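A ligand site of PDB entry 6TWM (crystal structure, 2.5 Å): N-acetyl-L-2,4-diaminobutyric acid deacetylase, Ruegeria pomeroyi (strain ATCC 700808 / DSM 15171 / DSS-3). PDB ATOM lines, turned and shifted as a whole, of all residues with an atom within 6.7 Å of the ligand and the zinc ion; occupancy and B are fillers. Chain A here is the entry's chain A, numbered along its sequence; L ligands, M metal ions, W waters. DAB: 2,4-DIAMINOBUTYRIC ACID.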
ATOM      1  N   ASN A  64       3.092  13.337   0.107  1.00  0.00           N
ATOM      2  CA  ASN A  64       2.550  13.842   1.365  1.00  0.00           C
ATOM      3  C   ASN A  64       1.030  13.778   1.326  1.00  0.00           C
ATOM      4  O   ASN A  64       0.386  13.257   2.235  1.00  0.00           O
ATOM      5  CB  ASN A  64       3.044  15.271   1.609  1.00  0.00           C
ATOM      6  CG  ASN A  64       2.594  15.856   2.940  1.00  0.00           C
ATOM      7  OD1 ASN A  64       1.626  15.412   3.553  1.00  0.00           O
ATOM      8  ND2 ASN A  64       3.308  16.878   3.395  1.00  0.00           N
ATOM      9  N   HIS A  65       0.440  14.303   0.253  1.00  0.00           N
ATOM     10  CA  HIS A  65      -0.936  14.011  -0.115  1.00  0.00           C
ATOM     11  C   HIS A  65      -0.917  12.956  -1.216  1.00  0.00           C
ATOM     12  O   HIS A  65      -0.093  13.011  -2.133  1.00  0.00           O
ATOM     13  CB  HIS A  65      -1.662  15.278  -0.594  1.00  0.00           C
ATOM     14  CG  HIS A  65      -1.742  16.345   0.447  1.00  0.00           C
ATOM     15  ND1 HIS A  65      -1.057  17.535   0.352  1.00  0.00           N
ATOM     16  CD2 HIS A  65      -2.434  16.401   1.610  1.00  0.00           C
ATOM     17  CE1 HIS A  65      -1.324  18.286   1.415  1.00  0.00           C
ATOM     18  NE2 HIS A  65      -2.162  17.615   2.186  1.00  0.00           N
ATOM     19  N   ASP A  67      -2.676  11.855  -3.823  1.00  0.00           N
ATOM     20  CA  ASP A  67      -3.038  11.973  -5.229  1.00  0.00           C
ATOM     21  C   ASP A  67      -2.197  12.999  -5.972  1.00  0.00           C
ATOM     22  O   ASP A  67      -2.686  13.698  -6.863  1.00  0.00           O
ATOM     23  CB  ASP A  67      -4.531  12.305  -5.363  1.00  0.00           C
ATOM     24  CG  ASP A  67      -4.917  13.588  -4.648  1.00  0.00           C
ATOM     25  OD1 ASP A  67      -4.066  14.164  -3.936  1.00  0.00           O
ATOM     26  OD2 ASP A  67      -6.079  14.033  -4.808  1.00  0.00           O
ATOM     27  N   GLU A  68      -0.913  13.099  -5.624  1.00  0.00           N
ATOM     28  CA  GLU A  68       0.006  14.045  -6.231  1.00  0.00           C
ATOM     29  C   GLU A  68       1.267  13.299  -6.634  1.00  0.00           C
ATOM     30  O   GLU A  68       1.935  12.711  -5.780  1.00  0.00           O
ATOM     31  CB  GLU A  68       0.316  15.194  -5.269  1.00  0.00           C
ATOM     32  CG  GLU A  68      -0.948  15.841  -4.725  1.00  0.00           C
ATOM     33  CD  GLU A  68      -0.680  16.842  -3.627  1.00  0.00           C
ATOM     34  OE1 GLU A  68       0.499  17.026  -3.262  1.00  0.00           O
ATOM     35  OE2 GLU A  68      -1.658  17.442  -3.137  1.00  0.00           O
ATOM     36  N   ARG A 107      -6.035  12.259  -1.396  1.00  0.00           N
ATOM     37  CA  ARG A 107      -5.291  13.231  -0.610  1.00  0.00           C
ATOM     38  C   ARG A 107      -5.050  12.748   0.812  1.00  0.00           C
ATOM     39  O   ARG A 107      -3.916  12.776   1.306  1.00  0.00           O
ATOM     40  CB  ARG A 107      -6.074  14.550  -0.604  1.00  0.00           C
ATOM     41  CG  ARG A 107      -5.446  15.709   0.147  1.00  0.00           C
ATOM     42  CD  ARG A 107      -6.271  16.964  -0.090  1.00  0.00           C
ATOM     43  NE  ARG A 107      -5.800  18.117   0.673  1.00  0.00           N
ATOM     44  CZ  ARG A 107      -4.811  18.916   0.285  1.00  0.00           C
ATOM     45  NH1 ARG A 107      -4.186  18.688  -0.856  1.00  0.00           N
ATOM     46  NH2 ARG A 107      -4.461  19.948   1.039  1.00  0.00           N
ATOM     47  N   ASN A 115      -5.067  14.101   7.141  1.00  0.00           N
ATOM     48  CA  ASN A 115      -4.263  14.968   6.292  1.00  0.00           C
ATOM     49  C   ASN A 115      -2.855  15.030   6.892  1.00  0.00           C
ATOM     50  O   ASN A 115      -2.655  15.609   7.965  1.00  0.00           O
ATOM     51  CB  ASN A 115      -4.901  16.349   6.208  1.00  0.00           C
ATOM     52  CG  ASN A 115      -4.153  17.297   5.287  1.00  0.00           C
ATOM     53  OD1 ASN A 115      -3.045  17.004   4.835  1.00  0.00           O
ATOM     54  ND2 ASN A 115      -4.761  18.433   4.993  1.00  0.00           N
ATOM     55  N   ASN A 117      -0.238  16.644   5.974  1.00  0.00           N
ATOM     56  CA  ASN A 117       0.311  17.989   6.044  1.00  0.00           C
ATOM     57  C   ASN A 117      -0.440  18.888   7.011  1.00  0.00           C
ATOM     58  O   ASN A 117      -0.245  20.108   6.983  1.00  0.00           O
ATOM     59  CB  ASN A 117       0.353  18.630   4.659  1.00  0.00           C
ATOM     60  CG  ASN A 117       1.521  19.598   4.501  1.00  0.00           C
ATOM     61  OD1 ASN A 117       2.467  19.578   5.294  1.00  0.00           O
ATOM     62  ND2 ASN A 117       1.457  20.453   3.488  1.00  0.00           N
ATOM     63  N   ARG A 118      -1.300  18.318   7.852  1.00  0.00           N
ATOM     64  CA  ARG A 118      -1.887  19.025   8.986  1.00  0.00           C
ATOM     65  C   ARG A 118      -1.691  18.245  10.280  1.00  0.00           C
ATOM     66  O   ARG A 118      -2.305  18.592  11.299  1.00  0.00           O
ATOM     67  CB  ARG A 118      -3.372  19.316   8.757  1.00  0.00           C
ATOM     68  CG  ARG A 118      -3.636  20.283   7.613  1.00  0.00           C
ATOM     69  CD  ARG A 118      -3.231  21.701   7.976  1.00  0.00           C
ATOM     70  NE  ARG A 118      -3.357  22.609   6.834  1.00  0.00           N
ATOM     71  CZ  ARG A 118      -3.047  23.897   6.852  1.00  0.00           C
ATOM     72  NH1 ARG A 118      -2.576  24.447   7.963  1.00  0.00           N
ATOM     73  NH2 ARG A 118      -3.197  24.644   5.762  1.00  0.00           N
ATOM     74  N   PHE A 150       7.547  17.128  -2.014  1.00  0.00           N
ATOM     75  CA  PHE A 150       6.849  17.409  -3.256  1.00  0.00           C
ATOM     76  C   PHE A 150       5.353  17.554  -3.028  1.00  0.00           C
ATOM     77  O   PHE A 150       4.750  16.860  -2.212  1.00  0.00           O
ATOM     78  CB  PHE A 150       7.111  16.295  -4.266  1.00  0.00           C
ATOM     79  CG  PHE A 150       8.450  16.397  -4.939  1.00  0.00           C
ATOM     80  CD1 PHE A 150       8.679  17.346  -5.914  1.00  0.00           C
ATOM     81  CD2 PHE A 150       9.465  15.524  -4.602  1.00  0.00           C
ATOM     82  CE1 PHE A 150       9.908  17.437  -6.531  1.00  0.00           C
ATOM     83  CE2 PHE A 150      10.699  15.608  -5.215  1.00  0.00           C
ATOM     84  CZ  PHE A 150      10.915  16.561  -6.189  1.00  0.00           C
ATOM     85  N   HIS A 151       4.744  18.449  -3.800  1.00  0.00           N
ATOM     86  CA  HIS A 151       3.303  18.660  -3.763  1.00  0.00           C
ATOM     87  C   HIS A 151       2.812  19.047  -5.148  1.00  0.00           C
ATOM     88  O   HIS A 151       3.528  19.665  -5.934  1.00  0.00           O
ATOM     89  CB  HIS A 151       2.921  19.748  -2.752  1.00  0.00           C
ATOM     90  CG  HIS A 151       3.041  19.326  -1.326  1.00  0.00           C
ATOM     91  ND1 HIS A 151       2.046  18.620  -0.677  1.00  0.00           N
ATOM     92  CD2 HIS A 151       4.029  19.502  -0.421  1.00  0.00           C
ATOM     93  CE1 HIS A 151       2.421  18.379   0.567  1.00  0.00           C
ATOM     94  NE2 HIS A 151       3.619  18.913   0.754  1.00  0.00           N
ATOM     95  N   SER A 152       1.569  18.659  -5.433  1.00  0.00           N
ATOM     96  CA  SER A 152       0.878  19.048  -6.651  1.00  0.00           C
ATOM     97  C   SER A 152      -0.572  19.352  -6.306  1.00  0.00           C
ATOM     98  O   SER A 152      -0.978  19.300  -5.138  1.00  0.00           O
ATOM     99  CB  SER A 152       1.000  17.961  -7.733  1.00  0.00           C
ATOM    100  OG  SER A 152       2.347  17.522  -7.844  1.00  0.00           O
ATOM    101  N   GLY A 153      -1.371  19.668  -7.321  1.00  0.00           N
ATOM    102  CA  GLY A 153      -2.727  20.133  -7.071  1.00  0.00           C
ATOM    103  C   GLY A 153      -3.649  19.068  -6.507  1.00  0.00           C
ATOM    104  O   GLY A 153      -4.576  19.381  -5.767  1.00  0.00           O
ATOM    105  N   GLY A 154      -3.408  17.807  -6.849  1.00  0.00           N
ATOM    106  CA  GLY A 154      -4.356  16.756  -6.521  1.00  0.00           C
ATOM    107  C   GLY A 154      -5.531  16.763  -7.488  1.00  0.00           C
ATOM    108  O   GLY A 154      -5.598  17.540  -8.437  1.00  0.00           O
ATOM    109  N   LEU A 157      -7.350  20.413  -7.630  1.00  0.00           N
ATOM    110  CA  LEU A 157      -6.664  21.649  -7.946  1.00  0.00           C
ATOM    111  C   LEU A 157      -5.655  21.404  -9.065  1.00  0.00           C
ATOM    112  O   LEU A 157      -5.204  20.278  -9.289  1.00  0.00           O
ATOM    113  CB  LEU A 157      -5.933  22.237  -6.730  1.00  0.00           C
ATOM    114  CG  LEU A 157      -6.752  22.819  -5.583  1.00  0.00           C
ATOM    115  CD1 LEU A 157      -5.827  23.297  -4.468  1.00  0.00           C
ATOM    116  CD2 LEU A 157      -7.614  23.964  -6.075  1.00  0.00           C
ATOM    117  N   PHE A 159      -2.129  23.581 -10.674  1.00  0.00           N
ATOM    118  CA  PHE A 159      -1.215  24.695 -10.464  1.00  0.00           C
ATOM    119  C   PHE A 159      -0.312  24.874 -11.668  1.00  0.00           C
ATOM    120  O   PHE A 159      -0.076  23.932 -12.427  1.00  0.00           O
ATOM    121  CB  PHE A 159      -0.332  24.462  -9.228  1.00  0.00           C
ATOM    122  CG  PHE A 159      -1.040  24.635  -7.911  1.00  0.00           C
ATOM    123  CD1 PHE A 159      -1.085  25.868  -7.284  1.00  0.00           C
ATOM    124  CD2 PHE A 159      -1.657  23.554  -7.292  1.00  0.00           C
ATOM    125  CE1 PHE A 159      -1.732  26.027  -6.066  1.00  0.00           C
ATOM    126  CE2 PHE A 159      -2.301  23.699  -6.076  1.00  0.00           C
ATOM    127  CZ  PHE A 159      -2.336  24.944  -5.465  1.00  0.00           C
ATOM    128  N   HIS A 166       8.562  30.217   2.063  1.00  0.00           N
ATOM    129  CA  HIS A 166       7.682  31.031   2.888  1.00  0.00           C
ATOM    130  C   HIS A 166       8.390  32.276   3.403  1.00  0.00           C
ATOM    131  O   HIS A 166       9.583  32.237   3.720  1.00  0.00           O
ATOM    132  CB  HIS A 166       7.147  30.230   4.075  1.00  0.00           C
ATOM    133  CG  HIS A 166       6.295  29.058   3.677  1.00  0.00           C
ATOM    134  ND1 HIS A 166       6.781  27.777   3.637  1.00  0.00           N
ATOM    135  CD2 HIS A 166       4.997  28.998   3.296  1.00  0.00           C
ATOM    136  CE1 HIS A 166       5.813  26.967   3.250  1.00  0.00           C
ATOM    137  NE2 HIS A 166       4.721  27.679   3.031  1.00  0.00           N
ATOM    138  N   LEU A 192       4.871  31.600  -0.992  1.00  0.00           N
ATOM    139  CA  LEU A 192       3.497  31.183  -0.754  1.00  0.00           C
ATOM    140  C   LEU A 192       2.904  31.923   0.438  1.00  0.00           C
ATOM    141  O   LEU A 192       3.549  32.052   1.485  1.00  0.00           O
ATOM    142  CB  LEU A 192       3.436  29.682  -0.501  1.00  0.00           C
ATOM    143  CG  LEU A 192       3.183  28.667  -1.620  1.00  0.00           C
ATOM    144  CD1 LEU A 192       3.385  27.254  -1.077  1.00  0.00           C
ATOM    145  CD2 LEU A 192       1.788  28.800  -2.182  1.00  0.00           C
ATOM    146  N   LEU A 193       1.662  32.369   0.294  1.00  0.00           N
ATOM    147  CA  LEU A 193       0.875  32.842   1.434  1.00  0.00           C
ATOM    148  C   LEU A 193       0.203  31.628   2.075  1.00  0.00           C
ATOM    149  O   LEU A 193      -1.002  31.384   1.941  1.00  0.00           O
ATOM    150  CB  LEU A 193      -0.142  33.896   1.021  1.00  0.00           C
ATOM    151  CG  LEU A 193      -0.786  34.733   2.138  1.00  0.00           C
ATOM    152  CD1 LEU A 193      -2.031  34.078   2.735  1.00  0.00           C
ATOM    153  CD2 LEU A 193       0.228  35.049   3.245  1.00  0.00           C
ATOM    154  N   GLU A 194       1.018  30.823   2.748  1.00  0.00           N
ATOM    155  CA  GLU A 194       0.507  29.701   3.526  1.00  0.00           C
ATOM    156  C   GLU A 194       0.418  30.069   4.999  1.00  0.00           C
ATOM    157  O   GLU A 194       0.980  29.418   5.871  1.00  0.00           O
ATOM    158  CB  GLU A 194       1.370  28.466   3.301  1.00  0.00           C
ATOM    159  CG  GLU A 194       0.697  27.170   3.730  1.00  0.00           C
ATOM    160  CD  GLU A 194      -0.493  26.811   2.869  1.00  0.00           C
ATOM    161  OE1 GLU A 194      -0.396  26.969   1.632  1.00  0.00           O
ATOM    162  OE2 GLU A 194      -1.523  26.398   3.432  1.00  0.00           O
ATOM    163  N   MET A 200       1.682  21.722   9.583  1.00  0.00           N
ATOM    164  CA  MET A 200       2.290  21.357   8.322  1.00  0.00           C
ATOM    165  C   MET A 200       3.708  20.814   8.519  1.00  0.00           C
ATOM    166  O   MET A 200       4.392  21.142   9.485  1.00  0.00           O
ATOM    167  CB  MET A 200       2.337  22.548   7.370  1.00  0.00           C
ATOM    168  CG  MET A 200       0.973  23.129   7.054  1.00  0.00           C
ATOM    169  SD  MET A 200       1.053  24.348   5.725  1.00  0.00           S
ATOM    170  CE  MET A 200       2.228  25.508   6.429  1.00  0.00           C
ATOM    171  N   ASP A 202       5.947  21.600   6.349  1.00  0.00           N
ATOM    172  CA  ASP A 202       6.617  22.876   6.116  1.00  0.00           C
ATOM    173  C   ASP A 202       7.045  23.514   7.435  1.00  0.00           C
ATOM    174  O   ASP A 202       8.228  23.829   7.640  1.00  0.00           O
ATOM    175  CB  ASP A 202       5.668  23.820   5.360  1.00  0.00           C
ATOM    176  CG  ASP A 202       5.188  23.229   4.045  1.00  0.00           C
ATOM    177  OD1 ASP A 202       5.894  23.384   3.033  1.00  0.00           O
ATOM    178  OD2 ASP A 202       4.098  22.608   4.032  1.00  0.00           O
ATOM    179  N   THR A 214       9.589  23.064  -1.181  1.00  0.00           N
ATOM    180  CA  THR A 214       8.222  22.631  -1.444  1.00  0.00           C
ATOM    181  C   THR A 214       7.803  23.127  -2.821  1.00  0.00           C
ATOM    182  O   THR A 214       8.341  24.114  -3.329  1.00  0.00           O
ATOM    183  CB  THR A 214       7.253  23.133  -0.361  1.00  0.00           C
ATOM    184  OG1 THR A 214       5.965  22.554  -0.569  1.00  0.00           O
ATOM    185  CG2 THR A 214       7.148  24.658  -0.410  1.00  0.00           C
ATOM    186  N   THR A 215       6.859  22.412  -3.428  1.00  0.00           N
ATOM    187  CA  THR A 215       6.488  22.664  -4.817  1.00  0.00           C
ATOM    188  C   THR A 215       4.972  22.619  -4.964  1.00  0.00           C
ATOM    189  O   THR A 215       4.247  22.220  -4.055  1.00  0.00           O
ATOM    190  CB  THR A 215       7.117  21.633  -5.765  1.00  0.00           C
ATOM    191  OG1 THR A 215       6.603  20.333  -5.455  1.00  0.00           O
ATOM    192  CG2 THR A 215       8.628  21.624  -5.650  1.00  0.00           C
ATOM    193  N   GLU A 216       4.509  23.055  -6.133  1.00  0.00           N
ATOM    194  CA  GLU A 216       3.175  22.752  -6.639  1.00  0.00           C
ATOM    195  C   GLU A 216       3.344  22.552  -8.136  1.00  0.00           C
ATOM    196  O   GLU A 216       3.405  23.516  -8.897  1.00  0.00           O
ATOM    197  CB  GLU A 216       2.166  23.855  -6.342  1.00  0.00           C
ATOM    198  CG  GLU A 216       1.775  23.998  -4.875  1.00  0.00           C
ATOM    199  CD  GLU A 216       1.040  22.781  -4.337  1.00  0.00           C
ATOM    200  OE1 GLU A 216       0.418  22.057  -5.140  1.00  0.00           O
ATOM    201  OE2 GLU A 216       1.099  22.555  -3.111  1.00  0.00           O
HETATM  202  N   DAB L   1      -1.528  22.482   1.280  1.00  0.00           N
HETATM  203  CA  DAB L   1      -1.621  23.076  -0.049  1.00  0.00           C
HETATM  204  C   DAB L   1      -1.855  22.032  -1.190  1.00  0.00           C
HETATM  205  O   DAB L   1      -2.774  22.249  -2.029  1.00  0.00           O
HETATM  206  CB  DAB L   1      -0.366  23.863  -0.415  1.00  0.00           C
HETATM  207  CG  DAB L   1       0.038  24.839   0.697  1.00  0.00           C
HETATM  208  ND  DAB L   1      -0.599  26.137   0.664  1.00  0.00           N
HETATM  209  OXT DAB L   1      -1.105  21.016  -1.204  1.00  0.00           O
HETATM  210 ZN    ZN M   1      -0.527  19.158  -1.751  1.00  0.00          ZN
HETATM  211  O   HOH W   1       3.012  23.800   1.298  1.00  0.00           O
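The zinc ion is bound by an oxygen (OXT) of the ligand (2.0 Å) and the side-chain carboxylate of Glu 68 (2.5 Å). Slightly farther from the zinc ion lies ND1 of His 65 (2.7 Å). Slightly farther from the zinc ion lies OE1 of Glu 68 (2.8 Å). Slightly farther from the zinc ion lies a ring nitrogen (ND1) of His 151 (2.8 Å).
An oxygen (OXT) of the ligand sits close to the side-chain carboxylate of Glu 216 (3.3 Å). Hydrophobic or aromatic side chains that line the ligand: His 65. Within 4 Å of the ligand: His 65, Arg 107, His 151, Glu 194 and Glu 216. Along chain A the residues within 4 Å of the ligand span positions 65 to 216.
Residues that only touch the zinc ion: Ser 152 (3.4 Å) and Arg 107 (3.8 Å). Within 4 Å of the zinc ion: His 65, Glu 68, Arg 107, His 151 and Ser 152.
The side-chain carboxylate of Glu 194 is in salt-bridge range of the guanidinium group of Arg 118, at 3.4 Å. The side-chain carboxylate (OE1) of Glu 68 lies close to a ring nitrogen (ND1) of His 151. OE1 of Glu 68 lies within hydrogen-bond range of N of Ser 152 (2.9 Å). OE2 of Glu 68 lies close to NH1 of Arg 107 (3.6 Å). A ring nitrogen (ND1) of His 65 lies within hydrogen-bond range of a ring nitrogen (ND1) of His 151 (3.4 Å). A ring nitrogen (NE2) of His 65 is in hydrogen-bond range of the guanidinium group (NH2) of Arg 107 (3.5 Å). The backbone NH (N) of His 151 sits at hydrogen-bond distance from the side-chain hydroxyl (OG1) of Thr 215, 3.1 Å away. NE2 of His 151 sits close to ND2 of Asn 64, 3.3 Å away.
A nitrogen (ND) of the ligand is covalently linked to the side-chain carboxylate of Glu 194, 1.3 Å away. The guanidinium group (NH1) of Arg 107 sits close to an oxygen (OXT) of the ligand, 3.9 Å away.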
